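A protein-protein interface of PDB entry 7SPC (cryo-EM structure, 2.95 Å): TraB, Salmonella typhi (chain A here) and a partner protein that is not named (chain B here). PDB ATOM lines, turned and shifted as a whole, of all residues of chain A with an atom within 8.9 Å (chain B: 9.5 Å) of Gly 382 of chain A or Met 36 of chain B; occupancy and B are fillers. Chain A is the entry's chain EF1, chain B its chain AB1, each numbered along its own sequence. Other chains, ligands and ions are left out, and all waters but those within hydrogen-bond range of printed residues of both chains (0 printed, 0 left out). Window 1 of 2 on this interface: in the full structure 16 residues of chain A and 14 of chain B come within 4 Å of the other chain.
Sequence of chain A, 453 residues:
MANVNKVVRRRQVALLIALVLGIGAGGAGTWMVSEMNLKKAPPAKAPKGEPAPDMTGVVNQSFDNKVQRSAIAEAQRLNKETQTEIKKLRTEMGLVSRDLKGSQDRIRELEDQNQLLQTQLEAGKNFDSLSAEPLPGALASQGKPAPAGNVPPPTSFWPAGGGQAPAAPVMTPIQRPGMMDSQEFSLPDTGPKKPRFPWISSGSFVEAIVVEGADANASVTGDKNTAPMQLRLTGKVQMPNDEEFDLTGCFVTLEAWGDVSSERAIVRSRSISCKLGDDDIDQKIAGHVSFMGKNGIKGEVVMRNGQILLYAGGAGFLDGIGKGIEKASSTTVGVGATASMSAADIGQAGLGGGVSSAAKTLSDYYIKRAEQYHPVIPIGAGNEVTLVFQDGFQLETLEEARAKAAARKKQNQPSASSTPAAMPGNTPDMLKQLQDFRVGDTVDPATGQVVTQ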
ATOM      1  N   ALA A 208      -8.410  28.382 -24.644  1.00  0.00           N
ATOM      2  CA  ALA A 208      -7.973  27.357 -23.710  1.00  0.00           C
ATOM      3  C   ALA A 208      -8.181  25.985 -24.334  1.00  0.00           C
ATOM      4  O   ALA A 208      -8.863  25.835 -25.348  1.00  0.00           O
ATOM      5  CB  ALA A 208      -8.717  27.463 -22.376  1.00  0.00           C
ATOM      6  N   ILE A 209      -7.582  24.978 -23.703  1.00  0.00           N
ATOM      7  CA  ILE A 209      -7.658  23.592 -24.148  1.00  0.00           C
ATOM      8  C   ILE A 209      -8.228  22.753 -23.014  1.00  0.00           C
ATOM      9  O   ILE A 209      -7.775  22.861 -21.866  1.00  0.00           O
ATOM     10  CB  ILE A 209      -6.282  23.060 -24.589  1.00  0.00           C
ATOM     11  CG1 ILE A 209      -5.995  23.467 -26.036  1.00  0.00           C
ATOM     12  CG2 ILE A 209      -6.209  21.550 -24.425  1.00  0.00           C
ATOM     13  CD1 ILE A 209      -5.045  22.546 -26.762  1.00  0.00           C
ATOM     14  N   VAL A 210      -9.221  21.924 -23.333  1.00  0.00           N
ATOM     15  CA  VAL A 210      -9.827  21.040 -22.346  1.00  0.00           C
ATOM     16  C   VAL A 210      -8.818  19.969 -21.953  1.00  0.00           C
ATOM     17  O   VAL A 210      -8.398  19.159 -22.786  1.00  0.00           O
ATOM     18  CB  VAL A 210     -11.114  20.409 -22.893  1.00  0.00           C
ATOM     19  CG1 VAL A 210     -11.837  19.645 -21.802  1.00  0.00           C
ATOM     20  CG2 VAL A 210     -12.016  21.475 -23.487  1.00  0.00           C
ATOM     21  N   VAL A 211      -8.426  19.960 -20.685  1.00  0.00           N
ATOM     22  CA  VAL A 211      -7.484  18.978 -20.169  1.00  0.00           C
ATOM     23  C   VAL A 211      -8.199  17.783 -19.554  1.00  0.00           C
ATOM     24  O   VAL A 211      -7.792  16.640 -19.758  1.00  0.00           O
ATOM     25  CB  VAL A 211      -6.527  19.642 -19.153  1.00  0.00           C
ATOM     26  CG1 VAL A 211      -5.730  18.592 -18.402  1.00  0.00           C
ATOM     27  CG2 VAL A 211      -5.597  20.608 -19.860  1.00  0.00           C
ATOM     28  N   GLU A 212      -9.275  18.025 -18.813  1.00  0.00           N
ATOM     29  CA  GLU A 212     -10.093  16.969 -18.233  1.00  0.00           C
ATOM     30  C   GLU A 212     -11.524  17.142 -18.720  1.00  0.00           C
ATOM     31  O   GLU A 212     -12.103  18.222 -18.573  1.00  0.00           O
ATOM     32  CB  GLU A 212     -10.025  17.007 -16.705  1.00  0.00           C
ATOM     33  CG  GLU A 212     -10.930  16.006 -16.009  1.00  0.00           C
ATOM     34  CD  GLU A 212     -11.191  16.371 -14.561  1.00  0.00           C
ATOM     35  OE1 GLU A 212     -11.646  15.494 -13.799  1.00  0.00           O
ATOM     36  OE2 GLU A 212     -10.939  17.534 -14.182  1.00  0.00           O
ATOM     37  N   GLY A 213     -12.083  16.089 -19.315  1.00  0.00           N
ATOM     38  CA  GLY A 213     -13.459  16.085 -19.752  1.00  0.00           C
ATOM     39  C   GLY A 213     -14.377  15.424 -18.742  1.00  0.00           C
ATOM     40  O   GLY A 213     -14.009  15.173 -17.593  1.00  0.00           O
ATOM     41  N   GLN A 230     -11.890  20.571 -15.705  1.00  0.00           N
ATOM     42  CA  GLN A 230     -10.924  21.666 -15.738  1.00  0.00           C
ATOM     43  C   GLN A 230     -10.154  21.700 -17.062  1.00  0.00           C
ATOM     44  O   GLN A 230     -10.046  20.703 -17.777  1.00  0.00           O
ATOM     45  CB  GLN A 230      -9.939  21.555 -14.576  1.00  0.00           C
ATOM     46  CG  GLN A 230      -8.938  20.425 -14.685  1.00  0.00           C
ATOM     47  CD  GLN A 230      -7.524  20.914 -14.468  1.00  0.00           C
ATOM     48  OE1 GLN A 230      -7.278  22.118 -14.402  1.00  0.00           O
ATOM     49  NE2 GLN A 230      -6.585  19.990 -14.352  1.00  0.00           N
ATOM     50  N   PHE A 291     -17.869  27.546 -27.034  1.00  0.00           N
ATOM     51  CA  PHE A 291     -17.311  26.680 -28.065  1.00  0.00           C
ATOM     52  C   PHE A 291     -17.819  27.154 -29.417  1.00  0.00           C
ATOM     53  O   PHE A 291     -19.025  27.110 -29.675  1.00  0.00           O
ATOM     54  CB  PHE A 291     -17.691  25.216 -27.824  1.00  0.00           C
ATOM     55  CG  PHE A 291     -17.227  24.290 -28.909  1.00  0.00           C
ATOM     56  CD1 PHE A 291     -15.880  24.054 -29.106  1.00  0.00           C
ATOM     57  CD2 PHE A 291     -18.141  23.659 -29.734  1.00  0.00           C
ATOM     58  CE1 PHE A 291     -15.455  23.208 -30.103  1.00  0.00           C
ATOM     59  CE2 PHE A 291     -17.717  22.814 -30.732  1.00  0.00           C
ATOM     60  CZ  PHE A 291     -16.371  22.586 -30.916  1.00  0.00           C
ATOM     61  N   ILE A 379     -17.718  14.969 -23.258  1.00  0.00           N
ATOM     62  CA  ILE A 379     -16.776  15.977 -23.726  1.00  0.00           C
ATOM     63  C   ILE A 379     -15.374  15.403 -23.573  1.00  0.00           C
ATOM     64  O   ILE A 379     -14.995  14.966 -22.480  1.00  0.00           O
ATOM     65  CB  ILE A 379     -16.912  17.298 -22.953  1.00  0.00           C
ATOM     66  CG1 ILE A 379     -18.348  17.824 -23.034  1.00  0.00           C
ATOM     67  CG2 ILE A 379     -15.939  18.337 -23.488  1.00  0.00           C
ATOM     68  CD1 ILE A 379     -18.817  18.122 -24.439  1.00  0.00           C
ATOM     69  N   GLY A 380     -14.610  15.408 -24.662  1.00  0.00           N
ATOM     70  CA  GLY A 380     -13.263  14.886 -24.642  1.00  0.00           C
ATOM     71  C   GLY A 380     -12.279  15.841 -23.997  1.00  0.00           C
ATOM     72  O   GLY A 380     -12.629  16.899 -23.480  1.00  0.00           O
ATOM     73  N   ALA A 381     -11.009  15.448 -24.037  1.00  0.00           N
ATOM     74  CA  ALA A 381      -9.931  16.194 -23.402  1.00  0.00           C
ATOM     75  C   ALA A 381      -8.916  16.688 -24.426  1.00  0.00           C
ATOM     76  O   ALA A 381      -7.719  16.758 -24.155  1.00  0.00           O
ATOM     77  CB  ALA A 381      -9.243  15.349 -22.336  1.00  0.00           C
ATOM     78  N   GLY A 382      -9.381  17.043 -25.620  1.00  0.00           N
ATOM     79  CA  GLY A 382      -8.482  17.538 -26.640  1.00  0.00           C
ATOM     80  C   GLY A 382      -9.082  18.638 -27.488  1.00  0.00           C
ATOM     81  O   GLY A 382      -8.621  18.890 -28.605  1.00  0.00           O
ATOM     82  N   ASN A 383     -10.111  19.295 -26.970  1.00  0.00           N
ATOM     83  CA  ASN A 383     -10.840  20.308 -27.717  1.00  0.00           C
ATOM     84  C   ASN A 383     -10.430  21.707 -27.275  1.00  0.00           C
ATOM     85  O   ASN A 383     -10.086  21.937 -26.114  1.00  0.00           O
ATOM     86  CB  ASN A 383     -12.347  20.127 -27.542  1.00  0.00           C
ATOM     87  CG  ASN A 383     -12.763  18.673 -27.583  1.00  0.00           C
ATOM     88  OD1 ASN A 383     -12.965  18.105 -28.654  1.00  0.00           O
ATOM     89  ND2 ASN A 383     -12.891  18.061 -26.414  1.00  0.00           N
ATOM     90  N   GLU A 384     -10.471  22.639 -28.221  1.00  0.00           N
ATOM     91  CA  GLU A 384     -10.157  24.038 -27.966  1.00  0.00           C
ATOM     92  C   GLU A 384     -11.446  24.797 -27.692  1.00  0.00           C
ATOM     93  O   GLU A 384     -12.405  24.700 -28.463  1.00  0.00           O
ATOM     94  CB  GLU A 384      -9.417  24.659 -29.149  1.00  0.00           C
ATOM     95  CG  GLU A 384      -8.325  23.779 -29.729  1.00  0.00           C
ATOM     96  CD  GLU A 384      -8.786  23.005 -30.948  1.00  0.00           C
ATOM     97  OE1 GLU A 384      -8.466  23.429 -32.078  1.00  0.00           O
ATOM     98  OE2 GLU A 384      -9.469  21.974 -30.777  1.00  0.00           O
ATOM     99  N   VAL A 385     -11.468  25.545 -26.593  1.00  0.00           N
ATOM    100  CA  VAL A 385     -12.630  26.304 -26.171  1.00  0.00           C
ATOM    101  C   VAL A 385     -12.176  27.706 -25.773  1.00  0.00           C
ATOM    102  O   VAL A 385     -11.003  28.055 -25.893  1.00  0.00           O
ATOM    103  CB  VAL A 385     -13.383  25.619 -25.012  1.00  0.00           C
ATOM    104  CG1 VAL A 385     -14.051  24.344 -25.491  1.00  0.00           C
ATOM    105  CG2 VAL A 385     -12.433  25.324 -23.871  1.00  0.00           C
ATOM    106  N   THR B  30     -18.937  19.624 -33.977  1.00  0.00           N
ATOM    107  CA  THR B  30     -18.935  18.977 -32.674  1.00  0.00           C
ATOM    108  C   THR B  30     -17.496  18.773 -32.228  1.00  0.00           C
ATOM    109  O   THR B  30     -16.555  18.870 -33.018  1.00  0.00           O
ATOM    110  CB  THR B  30     -19.666  17.630 -32.699  1.00  0.00           C
ATOM    111  OG1 THR B  30     -19.429  16.981 -33.954  1.00  0.00           O
ATOM    112  CG2 THR B  30     -21.160  17.816 -32.495  1.00  0.00           C
ATOM    113  N   THR B  31     -17.336  18.482 -30.941  1.00  0.00           N
ATOM    114  CA  THR B  31     -16.040  18.132 -30.392  1.00  0.00           C
ATOM    115  C   THR B  31     -15.688  16.693 -30.757  1.00  0.00           C
ATOM    116  O   THR B  31     -16.417  16.009 -31.480  1.00  0.00           O
ATOM    117  CB  THR B  31     -16.033  18.332 -28.879  1.00  0.00           C
ATOM    118  OG1 THR B  31     -17.002  17.469 -28.278  1.00  0.00           O
ATOM    119  CG2 THR B  31     -16.360  19.769 -28.538  1.00  0.00           C
ATOM    120  N   SER B  32     -14.555  16.222 -30.247  1.00  0.00           N
ATOM    121  CA  SER B  32     -14.070  14.882 -30.527  1.00  0.00           C
ATOM    122  C   SER B  32     -13.686  14.191 -29.226  1.00  0.00           C
ATOM    123  O   SER B  32     -13.700  14.788 -28.148  1.00  0.00           O
ATOM    124  CB  SER B  32     -12.871  14.914 -31.481  1.00  0.00           C
ATOM    125  OG  SER B  32     -11.972  15.950 -31.128  1.00  0.00           O
ATOM    126  N   ASP B  33     -13.344  12.910 -29.345  1.00  0.00           N
ATOM    127  CA  ASP B  33     -12.879  12.124 -28.203  1.00  0.00           C
ATOM    128  C   ASP B  33     -11.898  11.088 -28.745  1.00  0.00           C
ATOM    129  O   ASP B  33     -12.315  10.084 -29.332  1.00  0.00           O
ATOM    130  CB  ASP B  33     -14.040  11.470 -27.468  1.00  0.00           C
ATOM    131  CG  ASP B  33     -13.791  11.351 -25.977  1.00  0.00           C
ATOM    132  OD1 ASP B  33     -12.613  11.309 -25.568  1.00  0.00           O
ATOM    133  OD2 ASP B  33     -14.777  11.298 -25.212  1.00  0.00           O
ATOM    134  N   THR B  34     -10.605  11.342 -28.548  1.00  0.00           N
ATOM    135  CA  THR B  34      -9.546  10.468 -29.036  1.00  0.00           C
ATOM    136  C   THR B  34      -8.870   9.700 -27.908  1.00  0.00           C
ATOM    137  O   THR B  34      -7.735   9.239 -28.073  1.00  0.00           O
ATOM    138  CB  THR B  34      -8.512  11.275 -29.817  1.00  0.00           C
ATOM    139  OG1 THR B  34      -8.340  12.556 -29.198  1.00  0.00           O
ATOM    140  CG2 THR B  34      -8.969  11.472 -31.253  1.00  0.00           C
ATOM    141  N   CYS B  35      -9.541   9.562 -26.764  1.00  0.00           N
ATOM    142  CA  CYS B  35      -9.002   8.865 -25.597  1.00  0.00           C
ATOM    143  C   CYS B  35      -7.703   9.506 -25.115  1.00  0.00           C
ATOM    144  O   CYS B  35      -6.832   8.835 -24.559  1.00  0.00           O
ATOM    145  CB  CYS B  35      -8.786   7.378 -25.886  1.00  0.00           C
ATOM    146  SG  CYS B  35     -10.284   6.466 -26.310  1.00  0.00           S
ATOM    147  N   MET B  36      -7.569  10.812 -25.330  1.00  0.00           N
ATOM    148  CA  MET B  36      -6.342  11.508 -24.978  1.00  0.00           C
ATOM    149  C   MET B  36      -6.181  11.566 -23.465  1.00  0.00           C
ATOM    150  O   MET B  36      -7.109  11.941 -22.743  1.00  0.00           O
ATOM    151  CB  MET B  36      -6.350  12.916 -25.566  1.00  0.00           C
ATOM    152  CG  MET B  36      -5.016  13.628 -25.488  1.00  0.00           C
ATOM    153  SD  MET B  36      -5.103  15.314 -26.109  1.00  0.00           S
ATOM    154  CE  MET B  36      -5.874  15.037 -27.700  1.00  0.00           C
ATOM    155  N   THR B  37      -4.996  11.199 -22.989  1.00  0.00           N
ATOM    156  CA  THR B  37      -4.701  11.235 -21.570  1.00  0.00           C
ATOM    157  C   THR B  37      -4.573  12.683 -21.102  1.00  0.00           C
ATOM    158  O   THR B  37      -4.377  13.605 -21.896  1.00  0.00           O
ATOM    159  CB  THR B  37      -3.419  10.446 -21.288  1.00  0.00           C
ATOM    160  OG1 THR B  37      -3.531   9.148 -21.880  1.00  0.00           O
ATOM    161  CG2 THR B  37      -3.189  10.263 -19.799  1.00  0.00           C
ATOM    162  N   MET B  38      -4.716  12.879 -19.793  1.00  0.00           N
ATOM    163  CA  MET B  38      -4.597  14.212 -19.216  1.00  0.00           C
ATOM    164  C   MET B  38      -3.209  14.795 -19.449  1.00  0.00           C
ATOM    165  O   MET B  38      -3.071  15.979 -19.775  1.00  0.00           O
ATOM    166  CB  MET B  38      -4.912  14.143 -17.725  1.00  0.00           C
ATOM    167  CG  MET B  38      -5.407  15.427 -17.120  1.00  0.00           C
ATOM    168  SD  MET B  38      -6.539  15.076 -15.775  1.00  0.00           S
ATOM    169  CE  MET B  38      -6.664  16.685 -15.030  1.00  0.00           C
ATOM    170  N   THR B  39      -2.167  13.977 -19.284  1.00  0.00           N
ATOM    171  CA  THR B  39      -0.806  14.441 -19.539  1.00  0.00           C
ATOM    172  C   THR B  39      -0.608  14.779 -21.010  1.00  0.00           C
ATOM    173  O   THR B  39       0.047  15.776 -21.346  1.00  0.00           O
ATOM    174  CB  THR B  39       0.197  13.382 -19.086  1.00  0.00           C
ATOM    175  OG1 THR B  39       0.155  13.269 -17.660  1.00  0.00           O
ATOM    176  CG2 THR B  39       1.605  13.753 -19.509  1.00  0.00           C
ATOM    177  N   LYS B  40      -1.167  13.963 -21.904  1.00  0.00           N
ATOM    178  CA  LYS B  40      -1.076  14.261 -23.326  1.00  0.00           C
ATOM    179  C   LYS B  40      -1.774  15.575 -23.654  1.00  0.00           C
ATOM    180  O   LYS B  40      -1.270  16.371 -24.451  1.00  0.00           O
ATOM    181  CB  LYS B  40      -1.669  13.117 -24.143  1.00  0.00           C
ATOM    182  CG  LYS B  40      -1.012  11.770 -23.894  1.00  0.00           C
ATOM    183  CD  LYS B  40       0.166  11.532 -24.832  1.00  0.00           C
ATOM    184  CE  LYS B  40      -0.073  12.133 -26.207  1.00  0.00           C
ATOM    185  NZ  LYS B  40       1.190  12.271 -26.980  1.00  0.00           N
ATOM    186  N   ALA B  41      -2.937  15.819 -23.043  1.00  0.00           N
ATOM    187  CA  ALA B  41      -3.649  17.073 -23.267  1.00  0.00           C
ATOM    188  C   ALA B  41      -2.856  18.263 -22.747  1.00  0.00           C
ATOM    189  O   ALA B  41      -2.807  19.319 -23.391  1.00  0.00           O
ATOM    190  CB  ALA B  41      -5.020  17.015 -22.602  1.00  0.00           C
ATOM    191  N   ASN B  42      -2.239  18.119 -21.575  1.00  0.00           N
ATOM    192  CA  ASN B  42      -1.404  19.190 -21.041  1.00  0.00           C
ATOM    193  C   ASN B  42      -0.248  19.496 -21.983  1.00  0.00           C
ATOM    194  O   ASN B  42       0.050  20.667 -22.256  1.00  0.00           O
ATOM    195  CB  ASN B  42      -0.879  18.798 -19.662  1.00  0.00           C
ATOM    196  CG  ASN B  42      -0.682  19.987 -18.758  1.00  0.00           C
ATOM    197  OD1 ASN B  42      -1.482  20.915 -18.760  1.00  0.00           O
ATOM    198  ND2 ASN B  42       0.389  19.968 -17.977  1.00  0.00           N
ATOM    199  N   GLN B  43       0.409  18.456 -22.493  1.00  0.00           N
ATOM    200  CA  GLN B  43       1.517  18.654 -23.424  1.00  0.00           C
ATOM    201  C   GLN B  43       1.042  19.306 -24.717  1.00  0.00           C
ATOM    202  O   GLN B  43       1.726  20.173 -25.274  1.00  0.00           O
ATOM    203  CB  GLN B  43       2.205  17.322 -23.711  1.00  0.00           C
ATOM    204  CG  GLN B  43       3.607  17.458 -24.281  1.00  0.00           C
ATOM    205  CD  GLN B  43       4.370  18.620 -23.681  1.00  0.00           C
ATOM    206  OE1 GLN B  43       4.596  18.672 -22.474  1.00  0.00           O
ATOM    207  NE2 GLN B  43       4.772  19.564 -24.524  1.00  0.00           N
ATOM    208  N   LEU B  44      -0.118  18.888 -25.222  1.00  0.00           N
ATOM    209  CA  LEU B  44      -0.651  19.482 -26.442  1.00  0.00           C
ATOM    210  C   LEU B  44      -0.945  20.962 -26.249  1.00  0.00           C
ATOM    211  O   LEU B  44      -0.636  21.782 -27.121  1.00  0.00           O
ATOM    212  CB  LEU B  44      -1.911  18.732 -26.876  1.00  0.00           C
ATOM    213  CG  LEU B  44      -2.706  19.324 -28.036  1.00  0.00           C
ATOM    214  CD1 LEU B  44      -2.024  19.025 -29.360  1.00  0.00           C
ATOM    215  CD2 LEU B  44      -4.127  18.787 -28.029  1.00  0.00           C
ATOM    216  N   ALA B  45      -1.540  21.322 -25.111  1.00  0.00           N
ATOM    217  CA  ALA B  45      -1.809  22.728 -24.823  1.00  0.00           C
ATOM    218  C   ALA B  45      -0.519  23.523 -24.691  1.00  0.00           C
ATOM    219  O   ALA B  45      -0.428  24.664 -25.162  1.00  0.00           O
ATOM    220  CB  ALA B  45      -2.645  22.852 -23.551  1.00  0.00           C
ATOM    221  N   LYS B  48       0.778  24.125 -28.156  1.00  0.00           N
ATOM    222  CA  LYS B  48      -0.073  25.081 -28.913  1.00  0.00           C
ATOM    223  C   LYS B  48       0.329  26.497 -28.557  1.00  0.00           C
ATOM    224  O   LYS B  48       0.615  27.315 -29.476  1.00  0.00           O
ATOM    225  CB  LYS B  48      -1.554  24.963 -28.549  1.00  0.00           C
ATOM    226  CG  LYS B  48      -2.501  25.814 -29.379  1.00  0.00           C
ATOM    227  CD  LYS B  48      -3.945  25.410 -29.232  1.00  0.00           C
ATOM    228  CE  LYS B  48      -4.870  26.189 -30.140  1.00  0.00           C
ATOM    229  NZ  LYS B  48      -4.450  26.088 -31.558  1.00  0.00           N
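Gly 382 of chain A touches just one residue of chain B: Met 36. Met 36 of chain B touches just these residues of chain A: Ala 381 and Gly 382. Ala 381 of chain A touches two residues of chain B. Asn 383 of chain A touches just these residues of chain B: Thr 31 (3.1 Å) and Ser 32 (2.9 Å). Printed residues of chain A within 4 Å of Ser 32 of chain B: Gly 380 and Asn 383. Of the printed residues of chain A, Ala 45 of chain B touches Ile 209 (3.8 Å). Printed residues of chain B within 4 Å of Glu 212 of chain A: Met 38. Gln 43 of chain B touches none of the printed residues of chain A. The nearest residue of chain A that does not touch Met 36 of chain B is Val 211 of chain A (5.6 Å).
N of Ser 32 of chain B sits at hydrogen-bond distance from OD1 of Asn 383 of chain A (2.9 Å). O of Ala 381 of chain A lies close to SD of Met 36 of chain B.
SD of Met 36 of chain B sits close to N of Ala 41 of chain B (3.8 Å). The backbone NH of Val 210 of chain A is in hydrogen-bond range of the backbone carbonyl oxygen of Asn 383 of chain A (2.9 Å). O of Gln 230 of chain A sits at hydrogen-bond distance from N of Val 211 of chain A (3.4 Å). N of Glu 212 of chain A is in hydrogen-bond range of O of Gln 230 of chain A, at 3.0 Å. O of Gly 380 of chain A sits at hydrogen-bond distance from ND2 of Asn 383 of chain A (3.2 Å).
Among the printed residues, merely in contact across the chains: Asn 383 of chain A with Thr 31 of chain B (3.1 Å), Ala 381 of chain A with Ala 41 of chain B (3.1 Å), Gln 230 of chain A with Met 38 of chain B (3.4 Å), Val 211 of chain A with Met 38 of chain B (3.4 Å), Gly 380 of chain A with Ser 32 of chain B (3.5 Å), Phe 291 of chain A with Thr 31 of chain B (3.7 Å), Gly 380 of chain A with Asp 33 of chain B (3.8 Å), Gly 382 of chain A with Met 36 of chain B (3.8 Å), Glu 212 of chain A with Met 38 of chain B (3.8 Å), Ile 209 of chain A with Ala 45 of chain B (3.8 Å), Ile 209 of chain A with Lys 48 of chain B (3.9 Å) and Val 211 of chain A with Ala 41 of chain B (3.98 Å).
Of the 15 printed residues of chain A, 9 touch a printed residue of chain B. Printed residues of chain B that touch a printed residue of chain A: Thr 31, Ser 32, Asp 33, Met 36, Met 38, Ala 41, Ala 45 and Lys 48. Hydrophobic or aromatic side chains of chain B that line the printed part of chain A: Met 36, Met 38, Ala 41 and Ala 45. Among the printed residues, 14 pairs touch across the chains.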
